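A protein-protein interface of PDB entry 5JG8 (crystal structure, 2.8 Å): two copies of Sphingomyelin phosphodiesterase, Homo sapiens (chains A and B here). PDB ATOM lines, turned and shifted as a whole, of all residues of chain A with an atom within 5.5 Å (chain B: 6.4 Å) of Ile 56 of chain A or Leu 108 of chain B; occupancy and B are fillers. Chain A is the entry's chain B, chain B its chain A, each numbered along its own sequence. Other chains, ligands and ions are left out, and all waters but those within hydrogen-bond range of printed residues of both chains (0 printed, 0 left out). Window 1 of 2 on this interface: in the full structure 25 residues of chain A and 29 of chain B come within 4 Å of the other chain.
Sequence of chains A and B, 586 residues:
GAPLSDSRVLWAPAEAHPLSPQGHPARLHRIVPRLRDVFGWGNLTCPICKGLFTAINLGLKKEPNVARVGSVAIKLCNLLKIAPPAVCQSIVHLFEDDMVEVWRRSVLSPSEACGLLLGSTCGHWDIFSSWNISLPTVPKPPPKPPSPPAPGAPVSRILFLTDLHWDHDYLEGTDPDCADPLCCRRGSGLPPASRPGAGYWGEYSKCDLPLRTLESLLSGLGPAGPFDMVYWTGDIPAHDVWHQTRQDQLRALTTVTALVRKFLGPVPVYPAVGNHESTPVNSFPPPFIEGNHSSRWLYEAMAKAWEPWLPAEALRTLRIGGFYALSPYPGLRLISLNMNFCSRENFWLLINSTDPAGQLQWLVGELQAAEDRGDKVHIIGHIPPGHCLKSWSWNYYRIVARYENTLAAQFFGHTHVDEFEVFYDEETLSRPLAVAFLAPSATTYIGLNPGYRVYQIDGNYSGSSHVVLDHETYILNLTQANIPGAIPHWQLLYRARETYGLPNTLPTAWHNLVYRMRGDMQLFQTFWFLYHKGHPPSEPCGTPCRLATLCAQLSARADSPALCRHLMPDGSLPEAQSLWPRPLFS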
ATOM      1  N   GLY A  51      19.069   4.598  13.645  1.00  0.00           N
ATOM      2  CA  GLY A  51      20.139   3.691  14.024  1.00  0.00           C
ATOM      3  C   GLY A  51      21.475   4.401  14.119  1.00  0.00           C
ATOM      4  O   GLY A  51      22.263   4.150  15.037  1.00  0.00           O
ATOM      5  N   LEU A  52      21.738   5.312  13.182  1.00  0.00           N
ATOM      6  CA  LEU A  52      22.989   6.062  13.194  1.00  0.00           C
ATOM      7  C   LEU A  52      23.188   6.772  14.529  1.00  0.00           C
ATOM      8  O   LEU A  52      24.240   6.640  15.170  1.00  0.00           O
ATOM      9  CB  LEU A  52      22.990   7.064  12.036  1.00  0.00           C
ATOM     10  CG  LEU A  52      24.300   7.403  11.321  1.00  0.00           C
ATOM     11  CD1 LEU A  52      25.047   6.140  10.933  1.00  0.00           C
ATOM     12  CD2 LEU A  52      24.022   8.254  10.089  1.00  0.00           C
ATOM     13  N   PHE A  53      22.172   7.508  14.983  1.00  0.00           N
ATOM     14  CA  PHE A  53      22.318   8.261  16.221  1.00  0.00           C
ATOM     15  C   PHE A  53      22.182   7.393  17.465  1.00  0.00           C
ATOM     16  O   PHE A  53      22.631   7.807  18.538  1.00  0.00           O
ATOM     17  CB  PHE A  53      21.310   9.410  16.265  1.00  0.00           C
ATOM     18  CG  PHE A  53      21.683  10.559  15.381  1.00  0.00           C
ATOM     19  CD1 PHE A  53      22.577  11.519  15.814  1.00  0.00           C
ATOM     20  CD2 PHE A  53      21.153  10.672  14.109  1.00  0.00           C
ATOM     21  CE1 PHE A  53      22.933  12.574  14.999  1.00  0.00           C
ATOM     22  CE2 PHE A  53      21.504  11.726  13.290  1.00  0.00           C
ATOM     23  CZ  PHE A  53      22.395  12.679  13.737  1.00  0.00           C
ATOM     24  N   THR A  54      21.587   6.204  17.355  1.00  0.00           N
ATOM     25  CA  THR A  54      21.671   5.258  18.462  1.00  0.00           C
ATOM     26  C   THR A  54      23.109   4.785  18.651  1.00  0.00           C
ATOM     27  O   THR A  54      23.628   4.757  19.777  1.00  0.00           O
ATOM     28  CB  THR A  54      20.739   4.070  18.219  1.00  0.00           C
ATOM     29  OG1 THR A  54      19.379   4.522  18.176  1.00  0.00           O
ATOM     30  CG2 THR A  54      20.889   3.044  19.332  1.00  0.00           C
ATOM     31  N   ALA A  55      23.775   4.434  17.547  1.00  0.00           N
ATOM     32  CA  ALA A  55      25.170   4.017  17.621  1.00  0.00           C
ATOM     33  C   ALA A  55      26.064   5.150  18.108  1.00  0.00           C
ATOM     34  O   ALA A  55      27.009   4.918  18.871  1.00  0.00           O
ATOM     35  CB  ALA A  55      25.641   3.511  16.258  1.00  0.00           C
ATOM     36  N   ILE A  56      25.792   6.383  17.673  1.00  0.00           N
ATOM     37  CA  ILE A  56      26.561   7.515  18.183  1.00  0.00           C
ATOM     38  C   ILE A  56      26.334   7.664  19.682  1.00  0.00           C
ATOM     39  O   ILE A  56      27.279   7.827  20.463  1.00  0.00           O
ATOM     40  CB  ILE A  56      26.196   8.803  17.426  1.00  0.00           C
ATOM     41  CG1 ILE A  56      26.452   8.633  15.930  1.00  0.00           C
ATOM     42  CG2 ILE A  56      27.001   9.978  17.957  1.00  0.00           C
ATOM     43  CD1 ILE A  56      26.063   9.840  15.108  1.00  0.00           C
ATOM     44  N   ASN A  57      25.068   7.605  20.101  1.00  0.00           N
ATOM     45  CA  ASN A  57      24.717   7.702  21.514  1.00  0.00           C
ATOM     46  C   ASN A  57      25.525   6.716  22.350  1.00  0.00           C
ATOM     47  O   ASN A  57      26.336   7.109  23.200  1.00  0.00           O
ATOM     48  CB  ASN A  57      23.218   7.456  21.685  1.00  0.00           C
ATOM     49  CG  ASN A  57      22.752   7.667  23.108  1.00  0.00           C
ATOM     50  OD1 ASN A  57      22.981   6.828  23.980  1.00  0.00           O
ATOM     51  ND2 ASN A  57      22.076   8.785  23.348  1.00  0.00           N
ATOM     52  N   LEU A  58      25.314   5.416  22.120  1.00  0.00           N
ATOM     53  CA  LEU A  58      26.076   4.426  22.873  1.00  0.00           C
ATOM     54  C   LEU A  58      27.576   4.596  22.681  1.00  0.00           C
ATOM     55  O   LEU A  58      28.351   4.183  23.550  1.00  0.00           O
ATOM     56  CB  LEU A  58      25.666   3.007  22.471  1.00  0.00           C
ATOM     57  CG  LEU A  58      24.328   2.490  23.002  1.00  0.00           C
ATOM     58  CD1 LEU A  58      23.158   3.206  22.337  1.00  0.00           C
ATOM     59  CD2 LEU A  58      24.228   0.984  22.809  1.00  0.00           C
ATOM     60  N   GLY A  59      28.000   5.210  21.576  1.00  0.00           N
ATOM     61  CA  GLY A  59      29.424   5.354  21.326  1.00  0.00           C
ATOM     62  C   GLY A  59      30.072   6.366  22.250  1.00  0.00           C
ATOM     63  O   GLY A  59      31.117   6.099  22.849  1.00  0.00           O
ATOM     64  N   LEU A  60      29.462   7.541  22.382  1.00  0.00           N
ATOM     65  CA  LEU A  60      29.996   8.560  23.275  1.00  0.00           C
ATOM     66  C   LEU A  60      29.510   8.394  24.709  1.00  0.00           C
ATOM     67  O   LEU A  60      29.896   9.183  25.575  1.00  0.00           O
ATOM     68  CB  LEU A  60      29.653   9.964  22.756  1.00  0.00           C
ATOM     69  CG  LEU A  60      28.194  10.371  22.548  1.00  0.00           C
ATOM     70  CD1 LEU A  60      27.475  10.564  23.875  1.00  0.00           C
ATOM     71  CD2 LEU A  60      28.125  11.636  21.709  1.00  0.00           C
ATOM     72  N   LYS A  61      28.685   7.380  24.982  1.00  0.00           N
ATOM     73  CA  LYS A  61      28.364   7.042  26.362  1.00  0.00           C
ATOM     74  C   LYS A  61      29.563   6.485  27.127  1.00  0.00           C
ATOM     75  O   LYS A  61      29.479   6.340  28.352  1.00  0.00           O
ATOM     76  CB  LYS A  61      27.211   6.036  26.393  1.00  0.00           C
ATOM     77  CG  LYS A  61      26.691   5.719  27.781  1.00  0.00           C
ATOM     78  CD  LYS A  61      25.444   4.853  27.715  1.00  0.00           C
ATOM     79  CE  LYS A  61      25.033   4.380  29.097  1.00  0.00           C
ATOM     80  NZ  LYS A  61      24.681   5.518  29.990  1.00  0.00           N
ATOM     81  N   LEU A 108      21.489  15.021  20.472  1.00  0.00           N
ATOM     82  CA  LEU A 108      21.867  13.912  19.612  1.00  0.00           C
ATOM     83  C   LEU A 108      20.989  12.686  19.788  1.00  0.00           C
ATOM     84  O   LEU A 108      21.177  11.704  19.065  1.00  0.00           O
ATOM     85  CB  LEU A 108      23.328  13.534  19.868  1.00  0.00           C
ATOM     86  CG  LEU A 108      24.344  14.677  19.861  1.00  0.00           C
ATOM     87  CD1 LEU A 108      25.698  14.169  20.323  1.00  0.00           C
ATOM     88  CD2 LEU A 108      24.449  15.303  18.480  1.00  0.00           C
ATOM     89  N   LEU B  52      32.714  17.127  19.838  1.00  0.00           N
ATOM     90  CA  LEU B  52      31.676  16.104  19.900  1.00  0.00           C
ATOM     91  C   LEU B  52      31.533  15.381  18.564  1.00  0.00           C
ATOM     92  O   LEU B  52      31.508  14.144  18.508  1.00  0.00           O
ATOM     93  CB  LEU B  52      30.354  16.746  20.326  1.00  0.00           C
ATOM     94  CG  LEU B  52      29.411  15.893  21.172  1.00  0.00           C
ATOM     95  CD1 LEU B  52      30.163  15.247  22.315  1.00  0.00           C
ATOM     96  CD2 LEU B  52      28.282  16.756  21.709  1.00  0.00           C
ATOM     97  N   PHE B  53      31.433  16.137  17.472  1.00  0.00           N
ATOM     98  CA  PHE B  53      31.266  15.498  16.173  1.00  0.00           C
ATOM     99  C   PHE B  53      32.568  14.942  15.618  1.00  0.00           C
ATOM    100  O   PHE B  53      32.524  14.118  14.703  1.00  0.00           O
ATOM    101  CB  PHE B  53      30.624  16.470  15.183  1.00  0.00           C
ATOM    102  CG  PHE B  53      29.150  16.642  15.399  1.00  0.00           C
ATOM    103  CD1 PHE B  53      28.251  15.739  14.860  1.00  0.00           C
ATOM    104  CD2 PHE B  53      28.666  17.679  16.174  1.00  0.00           C
ATOM    105  CE1 PHE B  53      26.894  15.881  15.069  1.00  0.00           C
ATOM    106  CE2 PHE B  53      27.310  17.825  16.388  1.00  0.00           C
ATOM    107  CZ  PHE B  53      26.423  16.926  15.835  1.00  0.00           C
ATOM    108  N   THR B  54      33.720  15.378  16.130  1.00  0.00           N
ATOM    109  CA  THR B  54      34.963  14.682  15.812  1.00  0.00           C
ATOM    110  C   THR B  54      34.958  13.286  16.422  1.00  0.00           C
ATOM    111  O   THR B  54      35.310  12.298  15.760  1.00  0.00           O
ATOM    112  CB  THR B  54      36.165  15.484  16.312  1.00  0.00           C
ATOM    113  OG1 THR B  54      36.224  16.741  15.629  1.00  0.00           O
ATOM    114  CG2 THR B  54      37.454  14.719  16.058  1.00  0.00           C
ATOM    115  N   ILE B  56      32.274  11.615  17.225  1.00  0.00           N
ATOM    116  CA  ILE B  56      31.267  10.854  16.490  1.00  0.00           C
ATOM    117  C   ILE B  56      31.837  10.365  15.163  1.00  0.00           C
ATOM    118  O   ILE B  56      31.714   9.187  14.803  1.00  0.00           O
ATOM    119  CB  ILE B  56      30.004  11.707  16.279  1.00  0.00           C
ATOM    120  CG1 ILE B  56      29.441  12.163  17.625  1.00  0.00           C
ATOM    121  CG2 ILE B  56      28.961  10.928  15.501  1.00  0.00           C
ATOM    122  CD1 ILE B  56      28.225  13.048  17.510  1.00  0.00           C
ATOM    123  N   ASN B  57      32.472  11.271  14.420  1.00  0.00           N
ATOM    124  CA  ASN B  57      33.080  10.975  13.131  1.00  0.00           C
ATOM    125  C   ASN B  57      34.026   9.785  13.235  1.00  0.00           C
ATOM    126  O   ASN B  57      33.753   8.720  12.669  1.00  0.00           O
ATOM    127  CB  ASN B  57      33.814  12.215  12.609  1.00  0.00           C
ATOM    128  CG  ASN B  57      34.361  12.030  11.208  1.00  0.00           C
ATOM    129  OD1 ASN B  57      35.387  11.374  11.008  1.00  0.00           O
ATOM    130  ND2 ASN B  57      33.678  12.610  10.226  1.00  0.00           N
ATOM    131  N   LEU B  60      32.158   6.288  14.477  1.00  0.00           N
ATOM    132  CA  LEU B  60      31.407   5.430  13.569  1.00  0.00           C
ATOM    133  C   LEU B  60      32.194   5.039  12.324  1.00  0.00           C
ATOM    134  O   LEU B  60      31.653   4.340  11.460  1.00  0.00           O
ATOM    135  CB  LEU B  60      30.085   6.099  13.165  1.00  0.00           C
ATOM    136  CG  LEU B  60      30.088   7.466  12.479  1.00  0.00           C
ATOM    137  CD1 LEU B  60      30.615   7.383  11.055  1.00  0.00           C
ATOM    138  CD2 LEU B  60      28.685   8.045  12.498  1.00  0.00           C
ATOM    139  N   ASN B  65      29.932  -0.500  15.173  1.00  0.00           N
ATOM    140  CA  ASN B  65      28.822   0.440  15.280  1.00  0.00           C
ATOM    141  C   ASN B  65      27.988   0.432  14.007  1.00  0.00           C
ATOM    142  O   ASN B  65      26.757   0.521  14.065  1.00  0.00           O
ATOM    143  CB  ASN B  65      29.342   1.846  15.591  1.00  0.00           C
ATOM    144  CG  ASN B  65      30.057   1.927  16.934  1.00  0.00           C
ATOM    145  OD1 ASN B  65      29.773   1.152  17.849  1.00  0.00           O
ATOM    146  ND2 ASN B  65      30.976   2.879  17.059  1.00  0.00           N
ATOM    147  N   VAL B  69      23.921   0.111  13.819  1.00  0.00           N
ATOM    148  CA  VAL B  69      22.985   0.929  13.056  1.00  0.00           C
ATOM    149  C   VAL B  69      22.195   0.055  12.094  1.00  0.00           C
ATOM    150  O   VAL B  69      20.982   0.226  11.930  1.00  0.00           O
ATOM    151  CB  VAL B  69      23.728   2.061  12.318  1.00  0.00           C
ATOM    152  CG1 VAL B  69      24.709   2.754  13.253  1.00  0.00           C
ATOM    153  CG2 VAL B  69      24.429   1.539  11.076  1.00  0.00           C
ATOM    154  N   VAL B 100      26.371   5.165   5.847  1.00  0.00           N
ATOM    155  CA  VAL B 100      27.150   5.707   6.957  1.00  0.00           C
ATOM    156  C   VAL B 100      28.377   6.448   6.446  1.00  0.00           C
ATOM    157  O   VAL B 100      28.747   7.501   6.976  1.00  0.00           O
ATOM    158  CB  VAL B 100      27.536   4.585   7.937  1.00  0.00           C
ATOM    159  CG1 VAL B 100      28.653   5.048   8.853  1.00  0.00           C
ATOM    160  CG2 VAL B 100      26.322   4.155   8.747  1.00  0.00           C
ATOM    161  N   VAL B 102      28.761   8.220   3.695  1.00  0.00           N
ATOM    162  CA  VAL B 102      28.449   9.557   3.197  1.00  0.00           C
ATOM    163  C   VAL B 102      27.992  10.460   4.336  1.00  0.00           C
ATOM    164  O   VAL B 102      28.423  11.616   4.435  1.00  0.00           O
ATOM    165  CB  VAL B 102      27.408   9.489   2.063  1.00  0.00           C
ATOM    166  CG1 VAL B 102      27.859   8.503   0.996  1.00  0.00           C
ATOM    167  CG2 VAL B 102      26.031   9.134   2.601  1.00  0.00           C
ATOM    168  N   TRP B 103      27.120   9.961   5.216  1.00  0.00           N
ATOM    169  CA  TRP B 103      26.680  10.791   6.334  1.00  0.00           C
ATOM    170  C   TRP B 103      27.874  11.257   7.155  1.00  0.00           C
ATOM    171  O   TRP B 103      28.000  12.444   7.477  1.00  0.00           O
ATOM    172  CB  TRP B 103      25.686  10.024   7.205  1.00  0.00           C
ATOM    173  CG  TRP B 103      24.289  10.072   6.678  1.00  0.00           C
ATOM    174  CD1 TRP B 103      23.866   9.653   5.452  1.00  0.00           C
ATOM    175  CD2 TRP B 103      23.127  10.557   7.360  1.00  0.00           C
ATOM    176  NE1 TRP B 103      22.514   9.855   5.324  1.00  0.00           N
ATOM    177  CE2 TRP B 103      22.036  10.407   6.483  1.00  0.00           C
ATOM    178  CE3 TRP B 103      22.903  11.104   8.625  1.00  0.00           C
ATOM    179  CZ2 TRP B 103      20.742  10.783   6.831  1.00  0.00           C
ATOM    180  CZ3 TRP B 103      21.614  11.477   8.968  1.00  0.00           C
ATOM    181  CH2 TRP B 103      20.552  11.314   8.074  1.00  0.00           C
ATOM    182  N   ARG B 104      28.776  10.332   7.487  1.00  0.00           N
ATOM    183  CA  ARG B 104      29.993  10.698   8.204  1.00  0.00           C
ATOM    184  C   ARG B 104      30.772  11.769   7.454  1.00  0.00           C
ATOM    185  O   ARG B 104      31.320  12.691   8.069  1.00  0.00           O
ATOM    186  CB  ARG B 104      30.862   9.461   8.427  1.00  0.00           C
ATOM    187  CG  ARG B 104      32.173   9.752   9.126  1.00  0.00           C
ATOM    188  CD  ARG B 104      33.006   8.493   9.274  1.00  0.00           C
ATOM    189  NE  ARG B 104      33.381   7.937   7.977  1.00  0.00           N
ATOM    190  CZ  ARG B 104      34.399   8.377   7.245  1.00  0.00           C
ATOM    191  NH1 ARG B 104      35.145   9.384   7.678  1.00  0.00           N
ATOM    192  NH2 ARG B 104      34.671   7.813   6.077  1.00  0.00           N
ATOM    193  N   ARG B 105      30.850  11.661   6.126  1.00  0.00           N
ATOM    194  CA  ARG B 105      31.614  12.642   5.367  1.00  0.00           C
ATOM    195  C   ARG B 105      30.815  13.896   5.045  1.00  0.00           C
ATOM    196  O   ARG B 105      31.398  14.872   4.561  1.00  0.00           O
ATOM    197  CB  ARG B 105      32.144  12.033   4.065  1.00  0.00           C
ATOM    198  CG  ARG B 105      33.153  10.918   4.260  1.00  0.00           C
ATOM    199  CD  ARG B 105      33.674  10.394   2.930  1.00  0.00           C
ATOM    200  NE  ARG B 105      34.272  11.454   2.121  1.00  0.00           N
ATOM    201  CZ  ARG B 105      35.085  11.238   1.091  1.00  0.00           C
ATOM    202  NH1 ARG B 105      35.409   9.998   0.748  1.00  0.00           N
ATOM    203  NH2 ARG B 105      35.582  12.264   0.409  1.00  0.00           N
ATOM    204  N   SER B 106      29.503  13.897   5.282  1.00  0.00           N
ATOM    205  CA  SER B 106      28.699  15.063   4.939  1.00  0.00           C
ATOM    206  C   SER B 106      27.911  15.609   6.122  1.00  0.00           C
ATOM    207  O   SER B 106      28.299  16.610   6.735  1.00  0.00           O
ATOM    208  CB  SER B 106      27.718  14.714   3.821  1.00  0.00           C
ATOM    209  OG  SER B 106      26.705  13.850   4.312  1.00  0.00           O
ATOM    210  N   VAL B 107      26.810  14.933   6.460  1.00  0.00           N
ATOM    211  CA  VAL B 107      25.864  15.493   7.421  1.00  0.00           C
ATOM    212  C   VAL B 107      26.507  15.641   8.790  1.00  0.00           C
ATOM    213  O   VAL B 107      26.343  16.669   9.458  1.00  0.00           O
ATOM    214  CB  VAL B 107      24.593  14.628   7.492  1.00  0.00           C
ATOM    215  CG1 VAL B 107      23.671  15.138   8.590  1.00  0.00           C
ATOM    216  CG2 VAL B 107      23.879  14.615   6.146  1.00  0.00           C
ATOM    217  N   LEU B 108      27.250  14.629   9.232  1.00  0.00           N
ATOM    218  CA  LEU B 108      27.787  14.634  10.582  1.00  0.00           C
ATOM    219  C   LEU B 108      29.206  15.170  10.664  1.00  0.00           C
ATOM    220  O   LEU B 108      29.744  15.280  11.769  1.00  0.00           O
ATOM    221  CB  LEU B 108      27.744  13.218  11.160  1.00  0.00           C
ATOM    222  CG  LEU B 108      26.416  12.470  11.044  1.00  0.00           C
ATOM    223  CD1 LEU B 108      26.594  11.026  11.478  1.00  0.00           C
ATOM    224  CD2 LEU B 108      25.333  13.148  11.868  1.00  0.00           C
ATOM    225  N   SER B 109      29.833  15.483   9.538  1.00  0.00           N
ATOM    226  CA  SER B 109      31.208  15.954   9.569  1.00  0.00           C
ATOM    227  C   SER B 109      31.242  17.236  10.387  1.00  0.00           C
ATOM    228  O   SER B 109      30.574  18.210  10.006  1.00  0.00           O
ATOM    229  CB  SER B 109      31.745  16.209   8.164  1.00  0.00           C
ATOM    230  OG  SER B 109      30.943  17.154   7.475  1.00  0.00           O
ATOM    231  N   PRO B 110      31.950  17.291  11.522  1.00  0.00           N
ATOM    232  CA  PRO B 110      31.869  18.683  11.945  1.00  0.00           C
ATOM    233  C   PRO B 110      32.789  19.556  11.104  1.00  0.00           C
ATOM    234  O   PRO B 110      33.954  19.191  10.933  1.00  0.00           O
ATOM    235  CB  PRO B 110      32.350  18.621  13.392  1.00  0.00           C
ATOM    236  CG  PRO B 110      33.402  17.527  13.350  1.00  0.00           C
ATOM    237  CD  PRO B 110      32.906  16.511  12.328  1.00  0.00           C
ATOM    238  N   SER B 111      32.299  20.684  10.597  1.00  0.00           N
ATOM    239  CA  SER B 111      30.874  21.004  10.542  1.00  0.00           C
ATOM    240  C   SER B 111      30.745  21.998   9.391  1.00  0.00           C
ATOM    241  O   SER B 111      31.732  22.667   9.081  1.00  0.00           O
ATOM    242  CB  SER B 111      30.372  21.587  11.862  1.00  0.00           C
ATOM    243  OG  SER B 111      30.032  20.562  12.782  1.00  0.00           O
ATOM    244  N   GLU B 112      29.598  22.103   8.713  1.00  0.00           N
ATOM    245  CA  GLU B 112      28.408  21.253   8.830  1.00  0.00           C
ATOM    246  C   GLU B 112      27.682  21.265  10.172  1.00  0.00           C
ATOM    247  O   GLU B 112      27.261  22.323  10.634  1.00  0.00           O
ATOM    248  CB  GLU B 112      28.761  19.816   8.452  1.00  0.00           C
ATOM    249  CG  GLU B 112      29.309  19.681   7.032  1.00  0.00           C
ATOM    250  CD  GLU B 112      28.523  20.500   6.014  1.00  0.00           C
ATOM    251  OE1 GLU B 112      27.312  20.723   6.227  1.00  0.00           O
ATOM    252  OE2 GLU B 112      29.120  20.924   5.002  1.00  0.00           O
ATOM    253  N   ALA B 113      27.543  20.087  10.787  1.00  0.00           N
ATOM    254  CA  ALA B 113      26.538  19.887  11.832  1.00  0.00           C
ATOM    255  C   ALA B 113      26.519  21.035  12.837  1.00  0.00           C
ATOM    256  O   ALA B 113      25.456  21.585  13.148  1.00  0.00           O
ATOM    257  CB  ALA B 113      26.786  18.556  12.544  1.00  0.00           C
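The backbone carbonyl oxygen (O) of Trp 103 of chain B lies within hydrogen-bond range of the backbone NH (N) of Leu 108 of chain B (2.9 Å).
Val 69 of chain B touches Gly 51 of chain A. Leu 52 of chain A touches Val 69 of chain B. Val 100 of chain B touches Leu 52 of chain A (CG2 to CD1, 3.2 Å). Leu 108 of chain B touches Phe 53 of chain A (CD2 to CZ, 3.5 Å). Ala 55 of chain A touches Asn 65 of chain B. Val 69 of chain B touches Ala 55 of chain A (CG1 to CB, 3.2 Å). Ile 56 of chain B touches Ile 56 of chain A. CD1 of Ile 56 of chain A touches CD1 of Leu 108 of chain B, 3.9 Å away. Leu 108 of chain A touches Leu 52 of chain B. Leu 108 of chain A touches Ile 56 of chain B.
Ile 56 of chain A touches just these residues of chain B: Ile 56 (3.1 Å) and Leu 108 (3.9 Å). Of chain A, only Phe 53 and Ile 56 come within 4 Å of Leu 108 of chain B. Of the printed residues of chain B, Ala 55 of chain A touches Asn 65 (3.9 Å) and Val 69 (3.2 Å). Printed residues of chain A within 4 Å of Asn 65 of chain B: Ala 55. Of the printed residues of chain B, Leu 108 of chain A touches Leu 52, Phe 53 and Ile 56. Printed residues of chain B within 4 Å of Phe 53 of chain A: Leu 108 (3.5 Å). Printed residues of chain A within 4 Å of Val 100 of chain B: Leu 52 (3.2 Å). Val 102 of chain B touches none of the printed residues of chain A. Ala 113 of chain B touches none of the printed residues of chain A. The nearest residue of chain B that does not touch Ile 56 of chain A is Leu 60 of chain B (4.1 Å). The nearest printed residue of chain B that does not touch Phe 53 of chain A is Trp 103 of chain B (4.3 Å).
Printed residues of chain B that touch a printed residue of chain A: Leu 52, Phe 53, Ile 56, Asn 65, Val 69, Val 100, Trp 103 and Leu 108. Hydrophobic or aromatic side chains of chain B that line the printed part of chain A: Leu 52, Phe 53, Ile 56, Val 69, Val 100, Trp 103 and Leu 108. Hydrophobic or aromatic side chains of chain A within 4 Å of the printed part of chain B: Leu 52, Phe 53, Ala 55, Ile 56 and Leu 108. Among the printed residues, 12 pairs touch across the chains. Among the printed residues, no Asp or Glu carboxylate lies within 4 Å of a Lys or Arg side-chain nitrogen of the other chain.
Phe 53 of chain A touches Leu 108 of chain B, and with the chains exchanged Leu 108 of chain A touches Phe 53 of chain B. Ile 56 of chain B touches its own counterpart, Ile 56 of chain A. Ile 56 of chain A touches Leu 108 of chain B, and with the chains exchanged Leu 108 of chain A touches Ile 56 of chain B. Leu 108 of chain A touches Leu 52 of chain B, but with the chains exchanged Leu 52 of chain A does not touch Leu 108 of chain B (4.03 Å). Positions printed for both chains: 52, 53, 54, 56, 57, 60 and 108. Of the 12 pairs that touch across the chains among the printed residues, 5 have their exchanged pair printed and touching as well.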
